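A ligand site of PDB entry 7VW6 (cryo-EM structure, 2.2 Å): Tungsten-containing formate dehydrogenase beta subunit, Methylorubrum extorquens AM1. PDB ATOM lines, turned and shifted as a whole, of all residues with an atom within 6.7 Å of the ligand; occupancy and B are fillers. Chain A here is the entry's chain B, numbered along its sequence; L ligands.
Ile 330 touches the ligand.
Pro 348 touches the ligand (CG to S3, 3.9 Å).
CB of Ser 540 touches S1 of the ligand (3.8 Å).
Ile 541 touches the ligand.
Leu 544 touches the ligand (CB to S2, 3.9 Å).
Hydrophobic or aromatic side chains within 4 Å of the ligand: Ile 330, Pro 348, Ile 541 and Leu 544.
Of the 22 residues printed, 13 come within 4 Å of the ligand.
Along chain A the residues within 4 Å of the ligand span positions 330 to 545.
The nearest printed residue that does not touch the ligand is Arg 509 (4.2 Å).
SG of Cys 542 binds FE4 of the ligand.
The side-chain sulfur (SG) of Cys 505 binds an iron atom (FE2) of the ligand.
SG of Cys 508 is bound to FE3 of the ligand.
The backbone NH (N) of Cys 542 lies close to a sulfur (S1) of the ligand (3.7 Å).
An iron atom (FE1) of the ligand is bound by the side-chain sulfur (SG) of Cys 502 (2.3 Å).
A sulfur (S3) of the ligand lies close to the side-chain amide oxygen (OE1) of Gln 504.
The side-chain hydroxyl (OG) of Ser 501 sits close to a sulfur (S4) of the ligand (3.6 Å).
N of Gly 503 lies close to S4 of the ligand.
A sulfur (S4) of the ligand sits close to the backbone NH (N) of Cys 505, at 3.4 Å.
The backbone NH (N) of Cys 502 sits close to a sulfur (S2) of the ligand (3.6 Å).
A sulfur (S4) of the ligand sits close to the backbone NH (N) of Gln 504.
A sulfur (S1) of the ligand lies close to the backbone NH of Gly 545 (3.4 Å).
The side-chain amide nitrogen (NE2) of Gln 546 sits at hydrogen-bond distance from the backbone carbonyl oxygen (O) of Ile 541, 3.5 Å away.
The side-chain sulfur (SG) of Cys 502 sits close to the backbone NH (N) of Gln 504 (3.4 Å).
N of Gly 503 lies close to OG of Ser 501, 3.2 Å away.
The side-chain sulfur of Cys 508 sits close to the side-chain hydroxyl of Ser 501 (3.4 Å).
O of Gln 504 sits at hydrogen-bond distance from NH2 of Arg 509 (3.0 Å).
The backbone carbonyl oxygen (O) of Cys 508 sits at hydrogen-bond distance from the side-chain hydroxyl (OG1) of Thr 512 (2.8 Å).
The backbone NH (N) of Ile 541 sits close to the side-chain sulfur (SG) of Cys 505 (3.6 Å).
The side-chain amide oxygen (OE1) of Gln 504 lies close to the backbone carbonyl oxygen (O) of Pro 348, at 3.1 Å.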
ATOM      1  N   ILE A 330      13.131  34.946   0.116  1.00  0.00           N
ATOM      2  CA  ILE A 330      13.387  33.502   0.158  1.00  0.00           C
ATOM      3  C   ILE A 330      14.718  33.180   0.832  1.00  0.00           C
ATOM      4  O   ILE A 330      14.916  32.041   1.269  1.00  0.00           O
ATOM      5  CB  ILE A 330      13.315  32.913  -1.265  1.00  0.00           C
ATOM      6  CG1 ILE A 330      13.305  31.385  -1.231  1.00  0.00           C
ATOM      7  CG2 ILE A 330      14.474  33.419  -2.111  1.00  0.00           C
ATOM      8  CD1 ILE A 330      12.324  30.797  -0.252  1.00  0.00           C
ATOM      9  N   GLY A 346      19.928  32.179  -4.510  1.00  0.00           N
ATOM     10  CA  GLY A 346      19.265  31.652  -3.337  1.00  0.00           C
ATOM     11  C   GLY A 346      18.153  30.661  -3.660  1.00  0.00           C
ATOM     12  O   GLY A 346      16.978  30.961  -3.465  1.00  0.00           O
ATOM     13  N   LEU A 347      18.535  29.484  -4.140  1.00  0.00           N
ATOM     14  CA  LEU A 347      17.576  28.438  -4.489  1.00  0.00           C
ATOM     15  C   LEU A 347      17.572  27.376  -3.406  1.00  0.00           C
ATOM     16  O   LEU A 347      18.624  26.779  -3.143  1.00  0.00           O
ATOM     17  CB  LEU A 347      17.901  27.829  -5.841  1.00  0.00           C
ATOM     18  CG  LEU A 347      17.077  28.342  -7.017  1.00  0.00           C
ATOM     19  CD1 LEU A 347      17.261  29.837  -7.207  1.00  0.00           C
ATOM     20  CD2 LEU A 347      17.424  27.590  -8.295  1.00  0.00           C
ATOM     21  N   PRO A 348      16.427  27.104  -2.770  1.00  0.00           N
ATOM     22  CA  PRO A 348      16.400  26.093  -1.702  1.00  0.00           C
ATOM     23  C   PRO A 348      16.842  24.722  -2.187  1.00  0.00           C
ATOM     24  O   PRO A 348      16.527  24.309  -3.307  1.00  0.00           O
ATOM     25  CB  PRO A 348      14.936  26.094  -1.259  1.00  0.00           C
ATOM     26  CG  PRO A 348      14.411  27.409  -1.671  1.00  0.00           C
ATOM     27  CD  PRO A 348      15.141  27.793  -2.917  1.00  0.00           C
ATOM     28  N   GLU A 500       8.252  37.223  -4.871  1.00  0.00           N
ATOM     29  CA  GLU A 500       9.323  36.682  -4.043  1.00  0.00           C
ATOM     30  C   GLU A 500       9.663  35.228  -4.364  1.00  0.00           C
ATOM     31  O   GLU A 500      10.686  34.741  -3.876  1.00  0.00           O
ATOM     32  CB  GLU A 500       8.961  36.794  -2.558  1.00  0.00           C
ATOM     33  CG  GLU A 500       8.767  38.217  -2.061  1.00  0.00           C
ATOM     34  CD  GLU A 500      10.011  39.086  -2.198  1.00  0.00           C
ATOM     35  OE1 GLU A 500      11.134  38.557  -2.085  1.00  0.00           O
ATOM     36  OE2 GLU A 500       9.858  40.300  -2.407  1.00  0.00           O
ATOM     37  N   SER A 501       8.848  34.529  -5.149  1.00  0.00           N
ATOM     38  CA  SER A 501       9.125  33.143  -5.494  1.00  0.00           C
ATOM     39  C   SER A 501      10.470  33.040  -6.190  1.00  0.00           C
ATOM     40  O   SER A 501      10.777  33.816  -7.099  1.00  0.00           O
ATOM     41  CB  SER A 501       8.010  32.596  -6.400  1.00  0.00           C
ATOM     42  OG  SER A 501       8.454  31.482  -7.150  1.00  0.00           O
ATOM     43  N   CYS A 502      11.285  32.073  -5.766  1.00  0.00           N
ATOM     44  CA  CYS A 502      12.609  31.911  -6.369  1.00  0.00           C
ATOM     45  C   CYS A 502      12.523  31.396  -7.806  1.00  0.00           C
ATOM     46  O   CYS A 502      13.506  31.530  -8.549  1.00  0.00           O
ATOM     47  CB  CYS A 502      13.470  30.982  -5.520  1.00  0.00           C
ATOM     48  SG  CYS A 502      13.357  29.222  -5.883  1.00  0.00           S
ATOM     49  N   GLY A 503      11.395  30.810  -8.204  1.00  0.00           N
ATOM     50  CA  GLY A 503      11.196  30.351  -9.558  1.00  0.00           C
ATOM     51  C   GLY A 503      11.680  28.947  -9.854  1.00  0.00           C
ATOM     52  O   GLY A 503      11.650  28.540 -11.032  1.00  0.00           O
ATOM     53  N   GLN A 504      12.110  28.184  -8.851  1.00  0.00           N
ATOM     54  CA  GLN A 504      12.691  26.873  -9.111  1.00  0.00           C
ATOM     55  C   GLN A 504      11.649  25.872  -9.594  1.00  0.00           C
ATOM     56  O   GLN A 504      11.898  25.138 -10.553  1.00  0.00           O
ATOM     57  CB  GLN A 504      13.388  26.356  -7.852  1.00  0.00           C
ATOM     58  CG  GLN A 504      14.223  25.117  -8.086  1.00  0.00           C
ATOM     59  CD  GLN A 504      15.061  24.726  -6.888  1.00  0.00           C
ATOM     60  OE1 GLN A 504      14.804  25.141  -5.759  1.00  0.00           O
ATOM     61  NE2 GLN A 504      16.069  23.911  -7.127  1.00  0.00           N
ATOM     62  N   CYS A 505      10.490  25.805  -8.937  1.00  0.00           N
ATOM     63  CA  CYS A 505       9.553  24.714  -9.153  1.00  0.00           C
ATOM     64  C   CYS A 505       8.211  25.228  -9.698  1.00  0.00           C
ATOM     65  O   CYS A 505       7.771  26.332  -9.368  1.00  0.00           O
ATOM     66  CB  CYS A 505       9.325  23.900  -7.860  1.00  0.00           C
ATOM     67  SG  CYS A 505       8.514  24.754  -6.491  1.00  0.00           S
ATOM     68  N   THR A 506       7.580  24.393 -10.522  1.00  0.00           N
ATOM     69  CA  THR A 506       6.347  24.776 -11.211  1.00  0.00           C
ATOM     70  C   THR A 506       5.206  25.186 -10.277  1.00  0.00           C
ATOM     71  O   THR A 506       4.596  26.239 -10.525  1.00  0.00           O
ATOM     72  CB  THR A 506       5.895  23.644 -12.138  1.00  0.00           C
ATOM     73  OG1 THR A 506       6.995  23.176 -12.923  1.00  0.00           O
ATOM     74  CG2 THR A 506       4.765  24.107 -13.051  1.00  0.00           C
ATOM     75  N   PRO A 507       4.845  24.421  -9.242  1.00  0.00           N
ATOM     76  CA  PRO A 507       3.634  24.789  -8.467  1.00  0.00           C
ATOM     77  C   PRO A 507       3.699  26.181  -7.863  1.00  0.00           C
ATOM     78  O   PRO A 507       2.671  26.858  -7.783  1.00  0.00           O
ATOM     79  CB  PRO A 507       3.563  23.698  -7.394  1.00  0.00           C
ATOM     80  CG  PRO A 507       4.350  22.567  -7.941  1.00  0.00           C
ATOM     81  CD  PRO A 507       5.461  23.201  -8.700  1.00  0.00           C
ATOM     82  N   CYS A 508       4.878  26.625  -7.446  1.00  0.00           N
ATOM     83  CA  CYS A 508       5.045  27.938  -6.852  1.00  0.00           C
ATOM     84  C   CYS A 508       5.305  29.019  -7.898  1.00  0.00           C
ATOM     85  O   CYS A 508       4.686  30.079  -7.861  1.00  0.00           O
ATOM     86  CB  CYS A 508       6.197  27.901  -5.834  1.00  0.00           C
ATOM     87  SG  CYS A 508       6.671  29.484  -5.111  1.00  0.00           S
ATOM     88  N   ARG A 509       6.209  28.761  -8.842  1.00  0.00           N
ATOM     89  CA  ARG A 509       6.561  29.773  -9.846  1.00  0.00           C
ATOM     90  C   ARG A 509       5.351  30.128 -10.706  1.00  0.00           C
ATOM     91  O   ARG A 509       5.090  31.304 -10.977  1.00  0.00           O
ATOM     92  CB  ARG A 509       7.708  29.286 -10.715  1.00  0.00           C
ATOM     93  CG  ARG A 509       7.995  30.177 -11.924  1.00  0.00           C
ATOM     94  CD  ARG A 509       8.524  29.396 -13.115  1.00  0.00           C
ATOM     95  NE  ARG A 509       9.328  28.256 -12.702  1.00  0.00           N
ATOM     96  CZ  ARG A 509       9.082  27.006 -13.053  1.00  0.00           C
ATOM     97  NH1 ARG A 509       8.079  26.684 -13.848  1.00  0.00           N
ATOM     98  NH2 ARG A 509       9.868  26.040 -12.575  1.00  0.00           N
ATOM     99  N   THR A 512       1.569  30.859  -8.259  1.00  0.00           N
ATOM    100  CA  THR A 512       1.387  32.206  -7.733  1.00  0.00           C
ATOM    101  C   THR A 512       1.004  33.191  -8.833  1.00  0.00           C
ATOM    102  O   THR A 512       0.229  34.123  -8.592  1.00  0.00           O
ATOM    103  CB  THR A 512       2.651  32.684  -7.002  1.00  0.00           C
ATOM    104  OG1 THR A 512       3.766  32.709  -7.910  1.00  0.00           O
ATOM    105  CG2 THR A 512       2.974  31.771  -5.829  1.00  0.00           C
ATOM    106  N   SER A 540       4.840  21.842  -3.794  1.00  0.00           N
ATOM    107  CA  SER A 540       5.887  22.861  -3.760  1.00  0.00           C
ATOM    108  C   SER A 540       7.108  22.360  -2.996  1.00  0.00           C
ATOM    109  O   SER A 540       6.992  21.605  -2.031  1.00  0.00           O
ATOM    110  CB  SER A 540       5.376  24.158  -3.134  1.00  0.00           C
ATOM    111  OG  SER A 540       4.440  24.807  -3.976  1.00  0.00           O
ATOM    112  N   ILE A 541       8.294  22.794  -3.436  1.00  0.00           N
ATOM    113  CA  ILE A 541       9.536  22.296  -2.852  1.00  0.00           C
ATOM    114  C   ILE A 541       9.709  22.789  -1.428  1.00  0.00           C
ATOM    115  O   ILE A 541       9.972  22.007  -0.513  1.00  0.00           O
ATOM    116  CB  ILE A 541      10.733  22.682  -3.733  1.00  0.00           C
ATOM    117  CG1 ILE A 541      10.723  21.881  -5.039  1.00  0.00           C
ATOM    118  CG2 ILE A 541      12.041  22.457  -2.982  1.00  0.00           C
ATOM    119  CD1 ILE A 541      11.954  22.062  -5.887  1.00  0.00           C
ATOM    120  N   CYS A 542       9.552  24.096  -1.199  1.00  0.00           N
ATOM    121  CA  CYS A 542       9.892  24.698   0.085  1.00  0.00           C
ATOM    122  C   CYS A 542       8.677  25.372   0.707  1.00  0.00           C
ATOM    123  O   CYS A 542       7.579  25.380   0.160  1.00  0.00           O
ATOM    124  CB  CYS A 542      11.046  25.689  -0.069  1.00  0.00           C
ATOM    125  SG  CYS A 542      10.527  27.350  -0.535  1.00  0.00           S
ATOM    126  N   GLY A 543       8.914  25.975   1.880  1.00  0.00           N
ATOM    127  CA  GLY A 543       7.834  26.531   2.673  1.00  0.00           C
ATOM    128  C   GLY A 543       7.103  27.687   2.011  1.00  0.00           C
ATOM    129  O   GLY A 543       5.915  27.899   2.272  1.00  0.00           O
ATOM    130  N   LEU A 544       7.794  28.470   1.177  1.00  0.00           N
ATOM    131  CA  LEU A 544       7.153  29.613   0.534  1.00  0.00           C
ATOM    132  C   LEU A 544       5.992  29.161  -0.337  1.00  0.00           C
ATOM    133  O   LEU A 544       4.860  29.661  -0.202  1.00  0.00           O
ATOM    134  CB  LEU A 544       8.176  30.405  -0.277  1.00  0.00           C
ATOM    135  CG  LEU A 544       7.750  31.764  -0.876  1.00  0.00           C
ATOM    136  CD1 LEU A 544       8.945  32.684  -1.046  1.00  0.00           C
ATOM    137  CD2 LEU A 544       7.039  31.603  -2.206  1.00  0.00           C
ATOM    138  N   GLY A 545       6.242  28.212  -1.241  1.00  0.00           N
ATOM    139  CA  GLY A 545       5.175  27.720  -2.098  1.00  0.00           C
ATOM    140  C   GLY A 545       4.106  26.959  -1.332  1.00  0.00           C
ATOM    141  O   GLY A 545       2.927  27.025  -1.680  1.00  0.00           O
ATOM    142  N   GLN A 546       4.505  26.235  -0.289  1.00  0.00           N
ATOM    143  CA  GLN A 546       3.557  25.449   0.498  1.00  0.00           C
ATOM    144  C   GLN A 546       2.598  26.309   1.303  1.00  0.00           C
ATOM    145  O   GLN A 546       1.552  25.825   1.725  1.00  0.00           O
ATOM    146  CB  GLN A 546       4.310  24.509   1.438  1.00  0.00           C
ATOM    147  CG  GLN A 546       4.974  23.333   0.744  1.00  0.00           C
ATOM    148  CD  GLN A 546       6.019  22.664   1.613  1.00  0.00           C
ATOM    149  OE1 GLN A 546       6.053  22.868   2.827  1.00  0.00           O
ATOM    150  NE2 GLN A 546       6.867  21.859   1.001  1.00  0.00           N
HETATM  151 FE1  LIG L   1      11.408  28.383  -5.056  1.00  0.00          FE
HETATM  152 FE2  LIG L   1       9.725  26.229  -5.255  1.00  0.00          FE
HETATM  153 FE3  LIG L   1       8.723  28.660  -4.548  1.00  0.00          FE
HETATM  154 FE4  LIG L   1      10.327  27.286  -2.806  1.00  0.00          FE
HETATM  155  S1  LIG L   1       8.266  26.662  -3.559  1.00  0.00           S
HETATM  156  S2  LIG L   1      10.455  29.506  -3.313  1.00  0.00           S
HETATM  157  S3  LIG L   1      11.769  26.285  -4.257  1.00  0.00           S
HETATM  158  S4  LIG L   1       9.693  28.118  -6.533  1.00  0.00           S
